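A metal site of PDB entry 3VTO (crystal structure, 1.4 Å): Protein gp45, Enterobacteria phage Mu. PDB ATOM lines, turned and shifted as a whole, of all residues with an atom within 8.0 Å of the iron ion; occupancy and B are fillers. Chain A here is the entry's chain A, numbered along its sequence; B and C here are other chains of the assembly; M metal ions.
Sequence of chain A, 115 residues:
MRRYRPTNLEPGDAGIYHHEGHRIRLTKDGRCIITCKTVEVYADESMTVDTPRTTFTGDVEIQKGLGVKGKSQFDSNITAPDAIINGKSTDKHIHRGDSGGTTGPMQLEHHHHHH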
ATOM      1  N   THR A  90     -30.179 -19.704 -19.655  1.00  0.00           N
ATOM      2  CA  THR A  90     -29.018 -20.328 -20.266  1.00  0.00           C
ATOM      3  C   THR A  90     -29.456 -21.158 -21.502  1.00  0.00           C
ATOM      4  O   THR A  90     -28.832 -21.070 -22.547  1.00  0.00           O
ATOM      5  CB  THR A  90     -28.208 -21.211 -19.257  1.00  0.00           C
ATOM      6  OG1 THR A  90     -27.777 -20.398 -18.180  1.00  0.00           O
ATOM      7  CG2 THR A  90     -26.969 -21.805 -19.943  1.00  0.00           C
ATOM      8  N   HIS A  93     -30.155 -18.604 -24.414  1.00  0.00           N
ATOM      9  CA  HIS A  93     -29.329 -17.397 -24.557  1.00  0.00           C
ATOM     10  C   HIS A  93     -28.700 -17.307 -25.937  1.00  0.00           C
ATOM     11  O   HIS A  93     -28.468 -18.319 -26.601  1.00  0.00           O
ATOM     12  CB  HIS A  93     -28.238 -17.303 -23.498  1.00  0.00           C
ATOM     13  CG  HIS A  93     -27.001 -18.112 -23.798  1.00  0.00           C
ATOM     14  ND1 HIS A  93     -26.866 -19.446 -23.441  1.00  0.00           N
ATOM     15  CD2 HIS A  93     -25.814 -17.756 -24.377  1.00  0.00           C
ATOM     16  CE1 HIS A  93     -25.670 -19.870 -23.810  1.00  0.00           C
ATOM     17  NE2 HIS A  93     -25.020 -18.884 -24.399  1.00  0.00           N
ATOM     18  N   ILE A  94     -28.412 -16.064 -26.301  1.00  0.00           N
ATOM     19  CA  ILE A  94     -27.757 -15.744 -27.543  1.00  0.00           C
ATOM     20  C   ILE A  94     -26.572 -14.813 -27.264  1.00  0.00           C
ATOM     21  O   ILE A  94     -26.309 -14.455 -26.109  1.00  0.00           O
ATOM     22  CB  ILE A  94     -28.751 -15.069 -28.572  1.00  0.00           C
ATOM     23  CG1 ILE A  94     -29.191 -13.677 -28.088  1.00  0.00           C
ATOM     24  CG2 ILE A  94     -29.889 -16.006 -28.903  1.00  0.00           C
ATOM     25  CD1 ILE A  94     -30.051 -12.932 -29.119  1.00  0.00           C
ATOM     26  N   HIS A  95     -25.867 -14.440 -28.333  1.00  0.00           N
ATOM     27  CA  HIS A  95     -24.784 -13.439 -28.254  1.00  0.00           C
ATOM     28  C   HIS A  95     -24.881 -12.499 -29.449  1.00  0.00           C
ATOM     29  O   HIS A  95     -25.417 -12.897 -30.477  1.00  0.00           O
ATOM     30  CB  HIS A  95     -23.425 -14.131 -28.318  1.00  0.00           C
ATOM     31  CG  HIS A  95     -23.199 -15.147 -27.232  1.00  0.00           C
ATOM     32  ND1 HIS A  95     -22.438 -14.862 -26.119  1.00  0.00           N
ATOM     33  CD2 HIS A  95     -23.569 -16.453 -27.109  1.00  0.00           C
ATOM     34  CE1 HIS A  95     -22.393 -15.916 -25.321  1.00  0.00           C
ATOM     35  NE2 HIS A  95     -23.066 -16.900 -25.893  1.00  0.00           N
ATOM     36  N   THR A 103     -26.353 -14.344 -32.778  1.00  0.00           N
ATOM     37  CA  THR A 103     -26.279 -15.782 -32.927  1.00  0.00           C
ATOM     38  C   THR A 103     -27.645 -16.408 -32.657  1.00  0.00           C
ATOM     39  O   THR A 103     -28.588 -15.764 -32.209  1.00  0.00           O
ATOM     40  CB  THR A 103     -25.287 -16.384 -31.899  1.00  0.00           C
ATOM     41  OG1 THR A 103     -25.818 -16.286 -30.565  1.00  0.00           O
ATOM     42  CG2 THR A 103     -23.934 -15.721 -31.935  1.00  0.00           C
ATOM     43  N   GLY A 104     -27.758 -17.680 -32.963  1.00  0.00           N
ATOM     44  CA  GLY A 104     -28.883 -18.498 -32.482  1.00  0.00           C
ATOM     45  C   GLY A 104     -28.709 -18.883 -31.019  1.00  0.00           C
ATOM     46  O   GLY A 104     -27.705 -18.538 -30.387  1.00  0.00           O
ATOM     47  N   PRO A 105     -29.703 -19.587 -30.475  1.00  0.00           N
ATOM     48  CA  PRO A 105     -29.670 -19.972 -29.069  1.00  0.00           C
ATOM     49  C   PRO A 105     -28.682 -21.126 -28.764  1.00  0.00           C
ATOM     50  O   PRO A 105     -28.202 -21.782 -29.672  1.00  0.00           O
ATOM     51  CB  PRO A 105     -31.103 -20.421 -28.793  1.00  0.00           C
ATOM     52  CG  PRO A 105     -31.562 -20.913 -30.116  1.00  0.00           C
ATOM     53  CD  PRO A 105     -30.869 -20.166 -31.182  1.00  0.00           C
ATOM     54  N   MET A 106     -28.393 -21.344 -27.489  1.00  0.00           N
ATOM     55  CA  MET A 106     -27.456 -22.345 -27.059  1.00  0.00           C
ATOM     56  C   MET A 106     -27.796 -23.677 -27.717  1.00  0.00           C
ATOM     57  O   MET A 106     -28.953 -24.132 -27.701  1.00  0.00           O
ATOM     58  CB  MET A 106     -27.609 -22.498 -25.540  1.00  0.00           C
ATOM     59  CG  MET A 106     -26.745 -23.542 -24.918  1.00  0.00           C
ATOM     60  SD  MET A 106     -27.167 -23.797 -23.200  1.00  0.00           S
ATOM     61  CE  MET A 106     -25.867 -24.893 -22.689  1.00  0.00           C
ATOM     62  N   GLN A 107     -26.774 -24.309 -28.288  1.00  0.00           N
ATOM     63  CA  GLN A 107     -26.937 -25.580 -28.992  1.00  0.00           C
ATOM     64  C   GLN A 107     -25.969 -26.591 -28.424  1.00  0.00           C
ATOM     65  O   GLN A 107     -24.897 -26.244 -27.877  1.00  0.00           O
ATOM     66  CB  GLN A 107     -26.573 -25.394 -30.465  1.00  0.00           C
ATOM     67  CG  GLN A 107     -27.651 -24.828 -31.324  1.00  0.00           C
ATOM     68  CD  GLN A 107     -27.289 -24.878 -32.809  1.00  0.00           C
ATOM     69  OE1 GLN A 107     -26.218 -25.354 -33.201  1.00  0.00           O
ATOM     70  NE2 GLN A 107     -28.184 -24.377 -33.637  1.00  0.00           N
ATOM     71  N   THR B  90     -20.519 -17.928 -16.799  1.00  0.00           N
ATOM     72  CA  THR B  90     -21.645 -18.043 -17.712  1.00  0.00           C
ATOM     73  C   THR B  90     -22.203 -16.655 -18.072  1.00  0.00           C
ATOM     74  O   THR B  90     -22.425 -16.350 -19.258  1.00  0.00           O
ATOM     75  CB  THR B  90     -22.737 -18.945 -17.124  1.00  0.00           C
ATOM     76  OG1 THR B  90     -22.166 -20.227 -16.806  1.00  0.00           O
ATOM     77  CG2 THR B  90     -23.848 -19.140 -18.120  1.00  0.00           C
ATOM     78  N   HIS B  93     -19.647 -15.052 -20.608  1.00  0.00           N
ATOM     79  CA  HIS B  93     -18.892 -15.835 -21.571  1.00  0.00           C
ATOM     80  C   HIS B  93     -19.102 -15.398 -22.998  1.00  0.00           C
ATOM     81  O   HIS B  93     -20.130 -14.804 -23.343  1.00  0.00           O
ATOM     82  CB  HIS B  93     -19.203 -17.344 -21.474  1.00  0.00           C
ATOM     83  CG  HIS B  93     -20.485 -17.761 -22.153  1.00  0.00           C
ATOM     84  ND1 HIS B  93     -21.735 -17.675 -21.547  1.00  0.00           N
ATOM     85  CD2 HIS B  93     -20.702 -18.286 -23.383  1.00  0.00           C
ATOM     86  CE1 HIS B  93     -22.661 -18.092 -22.403  1.00  0.00           C
ATOM     87  NE2 HIS B  93     -22.050 -18.476 -23.508  1.00  0.00           N
ATOM     88  N   ILE B  94     -18.111 -15.730 -23.812  1.00  0.00           N
ATOM     89  CA  ILE B  94     -18.139 -15.416 -25.225  1.00  0.00           C
ATOM     90  C   ILE B  94     -17.823 -16.693 -26.023  1.00  0.00           C
ATOM     91  O   ILE B  94     -17.558 -17.762 -25.441  1.00  0.00           O
ATOM     92  CB  ILE B  94     -17.121 -14.352 -25.573  1.00  0.00           C
ATOM     93  CG1 ILE B  94     -15.658 -14.802 -25.296  1.00  0.00           C
ATOM     94  CG2 ILE B  94     -17.526 -13.060 -24.855  1.00  0.00           C
ATOM     95  CD1 ILE B  94     -14.575 -13.747 -25.583  1.00  0.00           C
ATOM     96  N   HIS B  95     -17.805 -16.553 -27.339  1.00  0.00           N
ATOM     97  CA  HIS B  95     -17.381 -17.651 -28.226  1.00  0.00           C
ATOM     98  C   HIS B  95     -16.516 -17.083 -29.373  1.00  0.00           C
ATOM     99  O   HIS B  95     -16.655 -15.893 -29.696  1.00  0.00           O
ATOM    100  CB  HIS B  95     -18.585 -18.358 -28.884  1.00  0.00           C
ATOM    101  CG  HIS B  95     -19.576 -18.888 -27.898  1.00  0.00           C
ATOM    102  ND1 HIS B  95     -19.683 -20.226 -27.578  1.00  0.00           N
ATOM    103  CD2 HIS B  95     -20.539 -18.259 -27.177  1.00  0.00           C
ATOM    104  CE1 HIS B  95     -20.650 -20.389 -26.677  1.00  0.00           C
ATOM    105  NE2 HIS B  95     -21.175 -19.204 -26.408  1.00  0.00           N
ATOM    106  N   THR B 103     -17.598 -13.286 -30.353  1.00  0.00           N
ATOM    107  CA  THR B 103     -18.924 -12.817 -30.058  1.00  0.00           C
ATOM    108  C   THR B 103     -18.864 -11.857 -28.877  1.00  0.00           C
ATOM    109  O   THR B 103     -17.866 -11.818 -28.125  1.00  0.00           O
ATOM    110  CB  THR B 103     -19.894 -13.951 -29.724  1.00  0.00           C
ATOM    111  OG1 THR B 103     -19.566 -14.511 -28.456  1.00  0.00           O
ATOM    112  CG2 THR B 103     -19.881 -15.015 -30.801  1.00  0.00           C
ATOM    113  N   GLY B 104     -19.986 -11.183 -28.664  1.00  0.00           N
ATOM    114  CA  GLY B 104     -20.208 -10.515 -27.384  1.00  0.00           C
ATOM    115  C   GLY B 104     -20.613 -11.490 -26.276  1.00  0.00           C
ATOM    116  O   GLY B 104     -20.755 -12.732 -26.507  1.00  0.00           O
ATOM    117  N   PRO B 105     -20.827 -10.976 -25.081  1.00  0.00           N
ATOM    118  CA  PRO B 105     -21.142 -11.797 -23.901  1.00  0.00           C
ATOM    119  C   PRO B 105     -22.576 -12.315 -23.927  1.00  0.00           C
ATOM    120  O   PRO B 105     -23.415 -11.813 -24.694  1.00  0.00           O
ATOM    121  CB  PRO B 105     -20.920 -10.819 -22.727  1.00  0.00           C
ATOM    122  CG  PRO B 105     -21.178  -9.508 -23.315  1.00  0.00           C
ATOM    123  CD  PRO B 105     -20.659  -9.542 -24.723  1.00  0.00           C
ATOM    124  N   MET B 106     -22.854 -13.303 -23.075  1.00  0.00           N
ATOM    125  CA  MET B 106     -24.181 -13.868 -22.950  1.00  0.00           C
ATOM    126  C   MET B 106     -25.254 -12.804 -22.862  1.00  0.00           C
ATOM    127  O   MET B 106     -25.164 -11.840 -22.062  1.00  0.00           O
ATOM    128  CB  MET B 106     -24.252 -14.729 -21.689  1.00  0.00           C
ATOM    129  CG  MET B 106     -25.592 -15.398 -21.488  1.00  0.00           C
ATOM    130  SD  MET B 106     -25.556 -16.212 -19.897  1.00  0.00           S
ATOM    131  CE  MET B 106     -27.100 -17.097 -19.975  1.00  0.00           C
ATOM    132  N   GLN B 107     -26.256 -12.942 -23.741  1.00  0.00           N
ATOM    133  CA  GLN B 107     -27.373 -12.011 -23.803  1.00  0.00           C
ATOM    134  C   GLN B 107     -28.707 -12.694 -23.592  1.00  0.00           C
ATOM    135  O   GLN B 107     -28.897 -13.903 -23.895  1.00  0.00           O
ATOM    136  CB  GLN B 107     -27.427 -11.307 -25.159  1.00  0.00           C
ATOM    137  CG  GLN B 107     -26.361 -10.276 -25.327  1.00  0.00           C
ATOM    138  CD  GLN B 107     -26.489  -9.494 -26.620  1.00  0.00           C
ATOM    139  OE1 GLN B 107     -27.287  -9.847 -27.492  1.00  0.00           O
ATOM    140  NE2 GLN B 107     -25.697  -8.448 -26.743  1.00  0.00           N
ATOM    141  N   THR C  90     -22.954 -26.931 -20.856  1.00  0.00           N
ATOM    142  CA  THR C  90     -22.659 -25.501 -20.860  1.00  0.00           C
ATOM    143  C   THR C  90     -21.185 -25.278 -21.219  1.00  0.00           C
ATOM    144  O   THR C  90     -20.836 -24.426 -22.042  1.00  0.00           O
ATOM    145  CB  THR C  90     -23.013 -24.854 -19.532  1.00  0.00           C
ATOM    146  OG1 THR C  90     -24.418 -24.999 -19.304  1.00  0.00           O
ATOM    147  CG2 THR C  90     -22.697 -23.360 -19.544  1.00  0.00           C
ATOM    148  N   HIS C  93     -20.907 -25.828 -25.082  1.00  0.00           N
ATOM    149  CA  HIS C  93     -21.976 -25.395 -25.986  1.00  0.00           C
ATOM    150  C   HIS C  93     -21.504 -24.437 -27.077  1.00  0.00           C
ATOM    151  O   HIS C  93     -20.513 -23.703 -26.928  1.00  0.00           O
ATOM    152  CB  HIS C  93     -23.159 -24.789 -25.202  1.00  0.00           C
ATOM    153  CG  HIS C  93     -22.988 -23.335 -24.881  1.00  0.00           C
ATOM    154  ND1 HIS C  93     -22.344 -22.908 -23.745  1.00  0.00           N
ATOM    155  CD2 HIS C  93     -23.396 -22.231 -25.533  1.00  0.00           C
ATOM    156  CE1 HIS C  93     -22.341 -21.583 -23.721  1.00  0.00           C
ATOM    157  NE2 HIS C  93     -22.955 -21.148 -24.814  1.00  0.00           N
ATOM    158  N   ILE C  94     -22.271 -24.427 -28.164  1.00  0.00           N
ATOM    159  CA  ILE C  94     -22.022 -23.578 -29.325  1.00  0.00           C
ATOM    160  C   ILE C  94     -23.331 -22.911 -29.720  1.00  0.00           C
ATOM    161  O   ILE C  94     -24.351 -23.103 -29.074  1.00  0.00           O
ATOM    162  CB  ILE C  94     -21.433 -24.386 -30.513  1.00  0.00           C
ATOM    163  CG1 ILE C  94     -22.442 -25.455 -31.012  1.00  0.00           C
ATOM    164  CG2 ILE C  94     -20.104 -24.997 -30.096  1.00  0.00           C
ATOM    165  CD1 ILE C  94     -21.937 -26.269 -32.206  1.00  0.00           C
ATOM    166  N   HIS C  95     -23.268 -22.084 -30.753  1.00  0.00           N
ATOM    167  CA  HIS C  95     -24.435 -21.416 -31.308  1.00  0.00           C
ATOM    168  C   HIS C  95     -24.323 -21.421 -32.819  1.00  0.00           C
ATOM    169  O   HIS C  95     -23.209 -21.428 -33.359  1.00  0.00           O
ATOM    170  CB  HIS C  95     -24.485 -19.910 -30.859  1.00  0.00           C
ATOM    171  CG  HIS C  95     -24.528 -19.723 -29.373  1.00  0.00           C
ATOM    172  ND1 HIS C  95     -25.702 -19.494 -28.691  1.00  0.00           N
ATOM    173  CD2 HIS C  95     -23.550 -19.755 -28.441  1.00  0.00           C
ATOM    174  CE1 HIS C  95     -25.446 -19.386 -27.391  1.00  0.00           C
ATOM    175  NE2 HIS C  95     -24.145 -19.507 -27.227  1.00  0.00           N
ATOM    176  N   THR C 103     -20.528 -21.123 -34.149  1.00  0.00           N
ATOM    177  CA  THR C 103     -19.487 -20.595 -33.290  1.00  0.00           C
ATOM    178  C   THR C 103     -18.670 -21.746 -32.690  1.00  0.00           C
ATOM    179  O   THR C 103     -19.081 -22.930 -32.808  1.00  0.00           O
ATOM    180  CB  THR C 103     -20.078 -19.790 -32.093  1.00  0.00           C
ATOM    181  OG1 THR C 103     -20.644 -20.709 -31.131  1.00  0.00           O
ATOM    182  CG2 THR C 103     -21.094 -18.774 -32.533  1.00  0.00           C
ATOM    183  N   GLY C 104     -17.531 -21.425 -32.097  1.00  0.00           N
ATOM    184  CA  GLY C 104     -16.811 -22.369 -31.232  1.00  0.00           C
ATOM    185  C   GLY C 104     -17.483 -22.515 -29.871  1.00  0.00           C
ATOM    186  O   GLY C 104     -18.515 -21.884 -29.586  1.00  0.00           O
ATOM    187  N   PRO C 105     -16.875 -23.321 -29.004  1.00  0.00           N
ATOM    188  CA  PRO C 105     -17.438 -23.570 -27.658  1.00  0.00           C
ATOM    189  C   PRO C 105     -17.250 -22.406 -26.693  1.00  0.00           C
ATOM    190  O   PRO C 105     -16.431 -21.497 -26.922  1.00  0.00           O
ATOM    191  CB  PRO C 105     -16.618 -24.756 -27.154  1.00  0.00           C
ATOM    192  CG  PRO C 105     -15.290 -24.626 -27.903  1.00  0.00           C
ATOM    193  CD  PRO C 105     -15.652 -24.077 -29.272  1.00  0.00           C
ATOM    194  N   MET C 106     -18.017 -22.450 -25.607  1.00  0.00           N
ATOM    195  CA  MET C 106     -17.947 -21.444 -24.551  1.00  0.00           C
ATOM    196  C   MET C 106     -16.499 -21.118 -24.182  1.00  0.00           C
ATOM    197  O   MET C 106     -15.719 -22.022 -23.896  1.00  0.00           O
ATOM    198  CB  MET C 106     -18.642 -22.024 -23.308  1.00  0.00           C
ATOM    199  CG  MET C 106     -18.680 -21.056 -22.146  1.00  0.00           C
ATOM    200  SD  MET C 106     -19.427 -21.896 -20.720  1.00  0.00           S
ATOM    201  CE  MET C 106     -19.569 -20.456 -19.634  1.00  0.00           C
ATOM    202  N   GLN C 107     -16.188 -19.815 -24.107  1.00  0.00           N
ATOM    203  CA  GLN C 107     -14.865 -19.345 -23.760  1.00  0.00           C
ATOM    204  C   GLN C 107     -14.942 -18.392 -22.615  1.00  0.00           C
ATOM    205  O   GLN C 107     -15.985 -17.752 -22.396  1.00  0.00           O
ATOM    206  CB  GLN C 107     -14.238 -18.589 -24.921  1.00  0.00           C
ATOM    207  CG  GLN C 107     -13.750 -19.427 -26.030  1.00  0.00           C
ATOM    208  CD  GLN C 107     -13.093 -18.561 -27.141  1.00  0.00           C
ATOM    209  OE1 GLN C 107     -13.146 -17.340 -27.111  1.00  0.00           O
ATOM    210  NE2 GLN C 107     -12.490 -19.214 -28.073  1.00  0.00           N
HETATM  211 FE    FE M   1     -23.076 -19.025 -25.381  1.00  0.00          FE
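The iron ion is bound by NE2 of His 95 of chain B, NE2 of His 93 of chain A, NE2 of His 95 of chain A, NE2 of His 95 of chain C, NE2 of His 93 of chain C and NE2 of His 93 of chain B.
The iron ion has six donor atoms within binding distance.
Six residues have an atom within 4 Å of the iron ion: His 93 of chain A, His 95 of chain A, His 93 of chain B, His 95 of chain B, His 93 of chain C and His 95 of chain C.
The nearest printed residue that does not touch the iron ion is Ile 94 of chain A (5.6 Å).
ND1 of His 95 of chain B is in hydrogen-bond range of N of Met 106 of chain C (3.4 Å).
A ring nitrogen (ND1) of His 95 of chain B is in hydrogen-bond range of the backbone carbonyl oxygen (O) of Gly 104 of chain C (2.9 Å).
N of Met 106 of chain B sits at hydrogen-bond distance from ND1 of His 95 of chain A (3.4 Å).
The backbone carbonyl oxygen (O) of His 95 of chain A sits at hydrogen-bond distance from the backbone NH (N) of Thr 103 of chain A, 2.9 Å away.
A ring nitrogen (ND1) of His 95 of chain C is in hydrogen-bond range of the backbone NH of Met 106 of chain A (3.5 Å).
The backbone carbonyl oxygen of His 95 of chain C lies within hydrogen-bond range of the backbone NH of Thr 103 of chain C (2.8 Å).
The backbone carbonyl oxygen (O) of His 93 of chain C is in hydrogen-bond range of the backbone NH (N) of Met 106 of chain C, at 3.1 Å.
A ring nitrogen (ND1) of His 93 of chain C sits at hydrogen-bond distance from the backbone carbonyl oxygen of Thr 90 of chain C, 2.7 Å away.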
